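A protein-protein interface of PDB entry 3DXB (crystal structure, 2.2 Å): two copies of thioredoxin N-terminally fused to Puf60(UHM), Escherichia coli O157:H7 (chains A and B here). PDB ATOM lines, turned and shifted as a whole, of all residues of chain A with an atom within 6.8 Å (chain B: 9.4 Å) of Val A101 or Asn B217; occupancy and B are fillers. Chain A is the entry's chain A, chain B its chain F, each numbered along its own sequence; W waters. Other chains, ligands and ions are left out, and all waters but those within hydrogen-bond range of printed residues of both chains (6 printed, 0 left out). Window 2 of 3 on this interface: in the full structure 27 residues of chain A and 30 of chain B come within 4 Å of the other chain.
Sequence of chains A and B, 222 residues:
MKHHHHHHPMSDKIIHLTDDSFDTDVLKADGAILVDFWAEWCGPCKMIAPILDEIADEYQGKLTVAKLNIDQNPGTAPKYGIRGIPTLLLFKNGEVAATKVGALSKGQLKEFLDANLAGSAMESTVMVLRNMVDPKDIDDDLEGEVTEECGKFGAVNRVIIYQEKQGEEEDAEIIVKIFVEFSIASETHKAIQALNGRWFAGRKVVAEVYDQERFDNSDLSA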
ATOM      1  N   TYR A  80       2.574  22.687  -8.076  1.00  0.00           N
ATOM      2  CA  TYR A  80       1.799  23.291  -9.154  1.00  0.00           C
ATOM      3  C   TYR A  80       0.312  22.968  -9.057  1.00  0.00           C
ATOM      4  O   TYR A  80      -0.444  23.220  -9.995  1.00  0.00           O
ATOM      5  CB  TYR A  80       2.362  22.873 -10.514  1.00  0.00           C
ATOM      6  CG  TYR A  80       3.720  23.460 -10.802  1.00  0.00           C
ATOM      7  CD1 TYR A  80       4.883  22.768 -10.465  1.00  0.00           C
ATOM      8  CD2 TYR A  80       3.847  24.715 -11.399  1.00  0.00           C
ATOM      9  CE1 TYR A  80       6.141  23.308 -10.720  1.00  0.00           C
ATOM     10  CE2 TYR A  80       5.101  25.266 -11.654  1.00  0.00           C
ATOM     11  CZ  TYR A  80       6.242  24.556 -11.313  1.00  0.00           C
ATOM     12  OH  TYR A  80       7.485  25.088 -11.564  1.00  0.00           O
ATOM     13  N   GLY A  81      -0.097  22.418  -7.916  1.00  0.00           N
ATOM     14  CA  GLY A  81      -1.496  22.096  -7.662  1.00  0.00           C
ATOM     15  C   GLY A  81      -2.037  21.011  -8.571  1.00  0.00           C
ATOM     16  O   GLY A  81      -3.207  21.053  -8.965  1.00  0.00           O
ATOM     17  N   ILE A  82      -1.180  20.050  -8.916  1.00  0.00           N
ATOM     18  CA  ILE A  82      -1.588  18.898  -9.714  1.00  0.00           C
ATOM     19  C   ILE A  82      -2.489  18.031  -8.848  1.00  0.00           C
ATOM     20  O   ILE A  82      -2.170  17.742  -7.696  1.00  0.00           O
ATOM     21  CB  ILE A  82      -0.368  18.077 -10.248  1.00  0.00           C
ATOM     22  CG1 ILE A  82       0.536  18.924 -11.169  1.00  0.00           C
ATOM     23  CG2 ILE A  82      -0.815  16.771 -10.935  1.00  0.00           C
ATOM     24  CD1 ILE A  82      -0.169  19.708 -12.266  1.00  0.00           C
ATOM     25  N   ARG A  83      -3.633  17.655  -9.401  1.00  0.00           N
ATOM     26  CA  ARG A  83      -4.591  16.827  -8.695  1.00  0.00           C
ATOM     27  C   ARG A  83      -4.709  15.490  -9.416  1.00  0.00           C
ATOM     28  O   ARG A  83      -4.053  14.518  -9.046  1.00  0.00           O
ATOM     29  CB  ARG A  83      -5.950  17.526  -8.621  1.00  0.00           C
ATOM     30  CG  ARG A  83      -5.975  18.805  -7.784  1.00  0.00           C
ATOM     31  CD  ARG A  83      -7.309  19.520  -7.966  1.00  0.00           C
ATOM     32  NE  ARG A  83      -8.408  18.796  -7.330  1.00  0.00           N
ATOM     33  CZ  ARG A  83      -9.663  18.765  -7.775  1.00  0.00           C
ATOM     34  NH1 ARG A  83     -10.014  19.412  -8.882  1.00  0.00           N
ATOM     35  NH2 ARG A  83     -10.574  18.074  -7.105  1.00  0.00           N
ATOM     36  N   GLY A  84      -5.546  15.454 -10.447  1.00  0.00           N
ATOM     37  CA  GLY A  84      -5.700  14.264 -11.269  1.00  0.00           C
ATOM     38  C   GLY A  84      -4.609  14.173 -12.314  1.00  0.00           C
ATOM     39  O   GLY A  84      -3.978  15.174 -12.652  1.00  0.00           O
ATOM     40  N   ILE A  85      -4.377  12.963 -12.816  1.00  0.00           N
ATOM     41  CA  ILE A  85      -3.442  12.749 -13.920  1.00  0.00           C
ATOM     42  C   ILE A  85      -4.119  12.006 -15.080  1.00  0.00           C
ATOM     43  O   ILE A  85      -5.009  11.184 -14.850  1.00  0.00           O
ATOM     44  CB  ILE A  85      -2.128  12.042 -13.474  1.00  0.00           C
ATOM     45  CG1 ILE A  85      -2.420  10.774 -12.666  1.00  0.00           C
ATOM     46  CG2 ILE A  85      -1.227  13.018 -12.698  1.00  0.00           C
ATOM     47  CD1 ILE A  85      -1.236   9.835 -12.558  1.00  0.00           C
ATOM     48  N   PRO A  86      -3.716  12.310 -16.332  1.00  0.00           N
ATOM     49  CA  PRO A  86      -2.677  13.279 -16.684  1.00  0.00           C
ATOM     50  C   PRO A  86      -3.134  14.735 -16.618  1.00  0.00           C
ATOM     51  O   PRO A  86      -4.319  15.031 -16.769  1.00  0.00           O
ATOM     52  CB  PRO A  86      -2.331  12.903 -18.128  1.00  0.00           C
ATOM     53  CG  PRO A  86      -3.589  12.354 -18.678  1.00  0.00           C
ATOM     54  CD  PRO A  86      -4.297  11.675 -17.530  1.00  0.00           C
ATOM     55  N   THR A  87      -2.178  15.622 -16.362  1.00  0.00           N
ATOM     56  CA  THR A  87      -2.376  17.062 -16.456  1.00  0.00           C
ATOM     57  C   THR A  87      -1.268  17.607 -17.347  1.00  0.00           C
ATOM     58  O   THR A  87      -0.102  17.221 -17.220  1.00  0.00           O
ATOM     59  CB  THR A  87      -2.344  17.756 -15.063  1.00  0.00           C
ATOM     60  OG1 THR A  87      -3.470  17.327 -14.288  1.00  0.00           O
ATOM     61  CG2 THR A  87      -2.406  19.278 -15.200  1.00  0.00           C
ATOM     62  N   LEU A  88      -1.650  18.480 -18.266  1.00  0.00           N
ATOM     63  CA  LEU A  88      -0.692  19.160 -19.110  1.00  0.00           C
ATOM     64  C   LEU A  88      -0.548  20.599 -18.641  1.00  0.00           C
ATOM     65  O   LEU A  88      -1.534  21.333 -18.562  1.00  0.00           O
ATOM     66  CB  LEU A  88      -1.129  19.097 -20.576  1.00  0.00           C
ATOM     67  CG  LEU A  88      -1.269  17.697 -21.193  1.00  0.00           C
ATOM     68  CD1 LEU A  88      -2.110  17.748 -22.466  1.00  0.00           C
ATOM     69  CD2 LEU A  88       0.091  17.059 -21.453  1.00  0.00           C
ATOM     70  N   LEU A  89       0.675  20.983 -18.290  1.00  0.00           N
ATOM     71  CA  LEU A  89       0.983  22.389 -18.039  1.00  0.00           C
ATOM     72  C   LEU A  89       1.807  22.924 -19.199  1.00  0.00           C
ATOM     73  O   LEU A  89       2.809  22.318 -19.587  1.00  0.00           O
ATOM     74  CB  LEU A  89       1.738  22.585 -16.721  1.00  0.00           C
ATOM     75  CG  LEU A  89       1.134  22.156 -15.378  1.00  0.00           C
ATOM     76  CD1 LEU A  89       1.954  22.761 -14.251  1.00  0.00           C
ATOM     77  CD2 LEU A  89      -0.326  22.544 -15.230  1.00  0.00           C
ATOM     78  N   THR A  99      -3.219  25.409 -18.974  1.00  0.00           N
ATOM     79  CA  THR A  99      -3.323  24.068 -18.398  1.00  0.00           C
ATOM     80  C   THR A  99      -4.417  23.248 -19.078  1.00  0.00           C
ATOM     81  O   THR A  99      -5.429  23.795 -19.532  1.00  0.00           O
ATOM     82  CB  THR A  99      -3.557  24.077 -16.858  1.00  0.00           C
ATOM     83  OG1 THR A  99      -4.931  24.363 -16.573  1.00  0.00           O
ATOM     84  CG2 THR A  99      -2.663  25.103 -16.151  1.00  0.00           C
ATOM     85  N   LYS A 100      -4.191  21.939 -19.155  1.00  0.00           N
ATOM     86  CA  LYS A 100      -5.203  20.995 -19.614  1.00  0.00           C
ATOM     87  C   LYS A 100      -5.214  19.742 -18.746  1.00  0.00           C
ATOM     88  O   LYS A 100      -4.214  19.036 -18.626  1.00  0.00           O
ATOM     89  CB  LYS A 100      -5.009  20.633 -21.088  1.00  0.00           C
ATOM     90  CG  LYS A 100      -6.040  19.632 -21.635  1.00  0.00           C
ATOM     91  CD  LYS A 100      -7.470  20.177 -21.617  1.00  0.00           C
ATOM     92  CE  LYS A 100      -7.754  21.092 -22.803  1.00  0.00           C
ATOM     93  NZ  LYS A 100      -9.137  21.663 -22.742  1.00  0.00           N
ATOM     94  N   VAL A 101      -6.371  19.475 -18.156  1.00  0.00           N
ATOM     95  CA  VAL A 101      -6.545  18.371 -17.222  1.00  0.00           C
ATOM     96  C   VAL A 101      -7.228  17.181 -17.922  1.00  0.00           C
ATOM     97  O   VAL A 101      -8.256  17.347 -18.575  1.00  0.00           O
ATOM     98  CB  VAL A 101      -7.300  18.895 -15.953  1.00  0.00           C
ATOM     99  CG1 VAL A 101      -8.458  18.006 -15.530  1.00  0.00           C
ATOM    100  CG2 VAL A 101      -6.317  19.167 -14.817  1.00  0.00           C
ATOM    101  N   GLY A 102      -6.626  15.997 -17.817  1.00  0.00           N
ATOM    102  CA  GLY A 102      -7.221  14.773 -18.359  1.00  0.00           C
ATOM    103  C   GLY A 102      -6.853  14.461 -19.800  1.00  0.00           C
ATOM    104  O   GLY A 102      -6.164  15.242 -20.461  1.00  0.00           O
ATOM    105  N   ALA A 103      -7.315  13.308 -20.284  1.00  0.00           N
ATOM    106  CA  ALA A 103      -7.023  12.860 -21.645  1.00  0.00           C
ATOM    107  C   ALA A 103      -7.834  13.644 -22.668  1.00  0.00           C
ATOM    108  O   ALA A 103      -8.872  14.223 -22.342  1.00  0.00           O
ATOM    109  CB  ALA A 103      -7.281  11.362 -21.788  1.00  0.00           C
ATOM    110  N   LEU A 104      -7.340  13.662 -23.901  1.00  0.00           N
ATOM    111  CA  LEU A 104      -8.001  14.350 -25.001  1.00  0.00           C
ATOM    112  C   LEU A 104      -7.456  13.873 -26.344  1.00  0.00           C
ATOM    113  O   LEU A 104      -6.336  13.375 -26.426  1.00  0.00           O
ATOM    114  CB  LEU A 104      -7.835  15.864 -24.866  1.00  0.00           C
ATOM    115  CG  LEU A 104      -6.502  16.478 -25.297  1.00  0.00           C
ATOM    116  CD1 LEU A 104      -6.518  17.978 -25.084  1.00  0.00           C
ATOM    117  CD2 LEU A 104      -5.349  15.845 -24.547  1.00  0.00           C
ATOM    118  N   VAL B 126     -11.778  28.821  -2.676  1.00  0.00           N
ATOM    119  CA  VAL B 126     -10.362  29.132  -2.693  1.00  0.00           C
ATOM    120  C   VAL B 126     -10.109  30.615  -2.442  1.00  0.00           C
ATOM    121  O   VAL B 126     -10.692  31.491  -3.090  1.00  0.00           O
ATOM    122  CB  VAL B 126      -9.710  28.706  -4.030  1.00  0.00           C
ATOM    123  CG1 VAL B 126      -8.184  28.762  -3.936  1.00  0.00           C
ATOM    124  CG2 VAL B 126     -10.175  27.302  -4.430  1.00  0.00           C
ATOM    125  N   ILE B 160      -1.556  25.649  -0.745  1.00  0.00           N
ATOM    126  CA  ILE B 160      -0.485  25.605  -1.743  1.00  0.00           C
ATOM    127  C   ILE B 160       0.408  26.839  -1.668  1.00  0.00           C
ATOM    128  O   ILE B 160      -0.055  27.976  -1.828  1.00  0.00           O
ATOM    129  CB  ILE B 160      -1.007  25.408  -3.198  1.00  0.00           C
ATOM    130  CG1 ILE B 160      -1.864  24.141  -3.300  1.00  0.00           C
ATOM    131  CG2 ILE B 160       0.170  25.340  -4.184  1.00  0.00           C
ATOM    132  CD1 ILE B 160      -2.531  23.939  -4.652  1.00  0.00           C
ATOM    133  N   GLU B 181      -7.624  26.525   0.105  1.00  0.00           N
ATOM    134  CA  GLU B 181      -8.913  25.978  -0.282  1.00  0.00           C
ATOM    135  C   GLU B 181      -9.641  25.459   0.953  1.00  0.00           C
ATOM    136  O   GLU B 181      -9.107  24.633   1.695  1.00  0.00           O
ATOM    137  CB  GLU B 181      -8.746  24.858  -1.319  1.00  0.00           C
ATOM    138  CG  GLU B 181     -10.007  24.029  -1.531  1.00  0.00           C
ATOM    139  CD  GLU B 181      -9.859  22.941  -2.575  1.00  0.00           C
ATOM    140  OE1 GLU B 181      -8.827  22.234  -2.581  1.00  0.00           O
ATOM    141  OE2 GLU B 181     -10.792  22.785  -3.388  1.00  0.00           O
ATOM    142  N   TYR B 210     -10.162  33.367  -5.344  1.00  0.00           N
ATOM    143  CA  TYR B 210      -9.524  32.883  -6.544  1.00  0.00           C
ATOM    144  C   TYR B 210     -10.551  32.016  -7.262  1.00  0.00           C
ATOM    145  O   TYR B 210     -11.287  31.275  -6.612  1.00  0.00           O
ATOM    146  CB  TYR B 210      -8.269  32.081  -6.192  1.00  0.00           C
ATOM    147  CG  TYR B 210      -7.414  31.783  -7.396  1.00  0.00           C
ATOM    148  CD1 TYR B 210      -6.516  32.730  -7.888  1.00  0.00           C
ATOM    149  CD2 TYR B 210      -7.514  30.560  -8.057  1.00  0.00           C
ATOM    150  CE1 TYR B 210      -5.734  32.462  -9.007  1.00  0.00           C
ATOM    151  CE2 TYR B 210      -6.743  30.286  -9.172  1.00  0.00           C
ATOM    152  CZ  TYR B 210      -5.857  31.238  -9.643  1.00  0.00           C
ATOM    153  OH  TYR B 210      -5.095  30.962 -10.754  1.00  0.00           O
ATOM    154  N   ASP B 211     -10.617  32.129  -8.587  1.00  0.00           N
ATOM    155  CA  ASP B 211     -11.534  31.308  -9.386  1.00  0.00           C
ATOM    156  C   ASP B 211     -11.352  29.824  -9.064  1.00  0.00           C
ATOM    157  O   ASP B 211     -10.253  29.273  -9.201  1.00  0.00           O
ATOM    158  CB  ASP B 211     -11.338  31.549 -10.885  1.00  0.00           C
ATOM    159  CG  ASP B 211     -12.417  30.888 -11.730  1.00  0.00           C
ATOM    160  OD1 ASP B 211     -13.494  31.492 -11.915  1.00  0.00           O
ATOM    161  OD2 ASP B 211     -12.187  29.766 -12.221  1.00  0.00           O
ATOM    162  N   GLN B 212     -12.437  29.199  -8.616  1.00  0.00           N
ATOM    163  CA  GLN B 212     -12.429  27.793  -8.216  1.00  0.00           C
ATOM    164  C   GLN B 212     -12.104  26.870  -9.388  1.00  0.00           C
ATOM    165  O   GLN B 212     -11.339  25.918  -9.234  1.00  0.00           O
ATOM    166  CB  GLN B 212     -13.776  27.408  -7.606  1.00  0.00           C
ATOM    167  CG  GLN B 212     -13.724  26.208  -6.687  1.00  0.00           C
ATOM    168  CD  GLN B 212     -15.096  25.818  -6.192  1.00  0.00           C
ATOM    169  OE1 GLN B 212     -15.826  25.080  -6.862  1.00  0.00           O
ATOM    170  NE2 GLN B 212     -15.457  26.311  -5.016  1.00  0.00           N
ATOM    171  N   GLU B 213     -12.680  27.163 -10.553  1.00  0.00           N
ATOM    172  CA  GLU B 213     -12.442  26.353 -11.747  1.00  0.00           C
ATOM    173  C   GLU B 213     -10.984  26.377 -12.212  1.00  0.00           C
ATOM    174  O   GLU B 213     -10.444  25.336 -12.601  1.00  0.00           O
ATOM    175  CB  GLU B 213     -13.381  26.742 -12.890  1.00  0.00           C
ATOM    176  CG  GLU B 213     -13.270  25.800 -14.089  1.00  0.00           C
ATOM    177  CD  GLU B 213     -14.417  25.920 -15.070  1.00  0.00           C
ATOM    178  OE1 GLU B 213     -14.473  25.085 -15.996  1.00  0.00           O
ATOM    179  OE2 GLU B 213     -15.257  26.837 -14.923  1.00  0.00           O
ATOM    180  N   ARG B 214     -10.353  27.552 -12.179  1.00  0.00           N
ATOM    181  CA  ARG B 214      -8.923  27.657 -12.468  1.00  0.00           C
ATOM    182  C   ARG B 214      -8.141  26.752 -11.519  1.00  0.00           C
ATOM    183  O   ARG B 214      -7.327  25.937 -11.957  1.00  0.00           O
ATOM    184  CB  ARG B 214      -8.430  29.109 -12.358  1.00  0.00           C
ATOM    185  CG  ARG B 214      -9.063  30.071 -13.357  1.00  0.00           C
ATOM    186  CD  ARG B 214      -8.506  31.484 -13.223  1.00  0.00           C
ATOM    187  NE  ARG B 214      -7.544  31.788 -14.278  1.00  0.00           N
ATOM    188  CZ  ARG B 214      -7.782  32.568 -15.329  1.00  0.00           C
ATOM    189  NH1 ARG B 214      -8.960  33.162 -15.487  1.00  0.00           N
ATOM    190  NH2 ARG B 214      -6.829  32.761 -16.228  1.00  0.00           N
ATOM    191  N   PHE B 215      -8.421  26.884 -10.223  1.00  0.00           N
ATOM    192  CA  PHE B 215      -7.744  26.112  -9.180  1.00  0.00           C
ATOM    193  C   PHE B 215      -7.966  24.603  -9.331  1.00  0.00           C
ATOM    194  O   PHE B 215      -7.015  23.824  -9.216  1.00  0.00           O
ATOM    195  CB  PHE B 215      -8.196  26.593  -7.797  1.00  0.00           C
ATOM    196  CG  PHE B 215      -7.522  25.888  -6.652  1.00  0.00           C
ATOM    197  CD1 PHE B 215      -6.258  26.276  -6.230  1.00  0.00           C
ATOM    198  CD2 PHE B 215      -8.161  24.847  -5.982  1.00  0.00           C
ATOM    199  CE1 PHE B 215      -5.632  25.628  -5.164  1.00  0.00           C
ATOM    200  CE2 PHE B 215      -7.544  24.194  -4.917  1.00  0.00           C
ATOM    201  CZ  PHE B 215      -6.277  24.586  -4.507  1.00  0.00           C
ATOM    202  N   ASP B 216      -9.214  24.207  -9.594  1.00  0.00           N
ATOM    203  CA  ASP B 216      -9.571  22.803  -9.815  1.00  0.00           C
ATOM    204  C   ASP B 216      -8.819  22.215 -10.999  1.00  0.00           C
ATOM    205  O   ASP B 216      -8.540  21.017 -11.030  1.00  0.00           O
ATOM    206  CB  ASP B 216     -11.076  22.651 -10.050  1.00  0.00           C
ATOM    207  CG  ASP B 216     -11.897  22.858  -8.788  1.00  0.00           C
ATOM    208  OD1 ASP B 216     -11.339  22.813  -7.671  1.00  0.00           O
ATOM    209  OD2 ASP B 216     -13.122  23.066  -8.924  1.00  0.00           O
ATOM    210  N   ASN B 217      -8.499  23.073 -11.966  1.00  0.00           N
ATOM    211  CA  ASN B 217      -7.786  22.682 -13.179  1.00  0.00           C
ATOM    212  C   ASN B 217      -6.286  22.984 -13.130  1.00  0.00           C
ATOM    213  O   ASN B 217      -5.626  23.036 -14.170  1.00  0.00           O
ATOM    214  CB  ASN B 217      -8.415  23.377 -14.391  1.00  0.00           C
ATOM    215  CG  ASN B 217      -9.755  22.785 -14.768  1.00  0.00           C
ATOM    216  OD1 ASN B 217      -9.824  21.802 -15.505  1.00  0.00           O
ATOM    217  ND2 ASN B 217     -10.830  23.389 -14.281  1.00  0.00           N
ATOM    218  N   SER B 218      -5.765  23.193 -11.920  1.00  0.00           N
ATOM    219  CA  SER B 218      -4.342  23.495 -11.690  1.00  0.00           C
ATOM    220  C   SER B 218      -3.839  24.778 -12.376  1.00  0.00           C
ATOM    221  O   SER B 218      -2.655  24.896 -12.705  1.00  0.00           O
ATOM    222  CB  SER B 218      -3.462  22.296 -12.061  1.00  0.00           C
ATOM    223  OG  SER B 218      -3.957  21.104 -11.480  1.00  0.00           O
ATOM    224  N   ASP B 219      -4.744  25.731 -12.586  1.00  0.00           N
ATOM    225  CA  ASP B 219      -4.382  27.050 -13.096  1.00  0.00           C
ATOM    226  C   ASP B 219      -4.224  27.988 -11.904  1.00  0.00           C
ATOM    227  O   ASP B 219      -5.211  28.496 -11.364  1.00  0.00           O
ATOM    228  CB  ASP B 219      -5.441  27.564 -14.087  1.00  0.00           C
ATOM    229  CG  ASP B 219      -5.108  28.942 -14.670  1.00  0.00           C
ATOM    230  OD1 ASP B 219      -4.069  29.546 -14.317  1.00  0.00           O
ATOM    231  OD2 ASP B 219      -5.910  29.427 -15.496  1.00  0.00           O
ATOM    232  N   LEU B 220      -2.973  28.194 -11.500  1.00  0.00           N
ATOM    233  CA  LEU B 220      -2.640  29.025 -10.341  1.00  0.00           C
ATOM    234  C   LEU B 220      -2.033  30.371 -10.757  1.00  0.00           C
ATOM    235  O   LEU B 220      -1.406  31.062  -9.944  1.00  0.00           O
ATOM    236  CB  LEU B 220      -1.694  28.263  -9.392  1.00  0.00           C
ATOM    237  CG  LEU B 220      -2.082  26.839  -8.950  1.00  0.00           C
ATOM    238  CD1 LEU B 220      -1.123  26.298  -7.904  1.00  0.00           C
ATOM    239  CD2 LEU B 220      -3.511  26.769  -8.432  1.00  0.00           C
ATOM    240  N   SER B 221      -2.258  30.749 -12.017  1.00  0.00           N
ATOM    241  CA  SER B 221      -1.582  31.889 -12.644  1.00  0.00           C
ATOM    242  C   SER B 221      -2.294  33.238 -12.519  1.00  0.00           C
ATOM    243  O   SER B 221      -1.715  34.274 -12.854  1.00  0.00           O
ATOM    244  CB  SER B 221      -1.337  31.597 -14.130  1.00  0.00           C
ATOM    245  OG  SER B 221      -2.532  31.727 -14.878  1.00  0.00           O
HETATM  246  O   HOH W   1      -4.589  18.569 -11.972  1.00  0.00           O
HETATM  247  O   HOH W   2      -8.491  21.456 -17.939  1.00  0.00           O
HETATM  248  O   HOH W   3     -10.167  21.133  -5.764  1.00  0.00           O
HETATM  249  O   HOH W   4      -4.930  22.748  -7.783  1.00  0.00           O
HETATM  250  O   HOH W   5      -7.769  20.585  -4.617  1.00  0.00           O
HETATM  251  O   HOH W   6      -0.012  24.732 -12.006  1.00  0.00           O
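OG of Ser B218 is in hydrogen-bond range of O of Gly A81 (2.6 Å). OD1 of Asp B216 is in salt-bridge range of NH1 of Arg A83. O of Asn B217 lies within hydrogen-bond range of OG1 of Thr A99 (2.8 Å).
The side-chain amide nitrogen of Asn B217 is in hydrogen-bond range of the backbone carbonyl oxygen of Glu B213 (2.6 Å).
O of Tyr A80 touches CB of Ser B218, at 3.8 Å. Tyr A80 touches Leu B220 (O to CD1, 3.8 Å). CA of Gly A81 touches CD1 of Ile B160, at 3.7 Å. CA of Ile A82 touches OG of Ser B218, at 3.7 Å. Thr A99 touches Ser B218 (CG2 to O, 3.5 Å). Asn B217 touches Val A101.
Of the printed residues of chain B, Tyr A80 touches Ser B218 and Leu B220. Printed residues of chain B within 4 Å of Arg A83: Asp B216 (3.1 Å). Of the printed residues of chain B, Thr A99 touches Asn B217 (2.8 Å) and Ser B218 (3.5 Å). Val A101 touches one residue of chain B. Asn B217 touches two residues of chain A. Of the printed residues of chain A, Ser B218 touches Tyr A80, Gly A81, Ile A82 and Thr A99. Of the printed residues of chain A, Leu B220 touches Tyr A80 (3.8 Å). The nearest printed residue of chain B that does not touch Thr A99 is Asp B219 (4.01 Å).
Printed residues of chain B that touch a printed residue of chain A: Ile B160, Asp B216, Asn B217, Ser B218 and Leu B220. Hydrophobic or aromatic side chains of chain B within 4 Å of the printed part of chain A: Ile B160 and Leu B220. Along chain A the printed residues that touch a printed residue of chain B span positions 80 to 101. Among the printed residues, Asp or Glu carboxylates within 4 Å of a Lys or Arg side-chain nitrogen of the other chain: Arg A83 with Asp B216 (3.8 Å).
No position is printed for both chains.
Water W6 bridges O of Tyr A80 and O of Ser B218. Water W1 lies within hydrogen-bond range of OG of Ser B218, OG1 of Thr A87 and N of Arg A83. Water W4 bridges the backbone carbonyl oxygen (O) of Gly A81 (2.7 Å) and the backbone carbonyl oxygen (O) of Phe B215 (2.7 Å). Water W2 bridges OD1 of Asn B217 (2.8 Å) and N of Val A101 (2.9 Å). Water W3 lies within hydrogen-bond range of the side-chain carboxylate of Asp B216 (2.8 Å), the side-chain carboxylate of Glu B181 (3.0 Å) and the guanidinium group of Arg A83 (3.3 Å). Water W5 bridges the side-chain carboxylate of Glu B181 and the guanidinium group of Arg A83.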
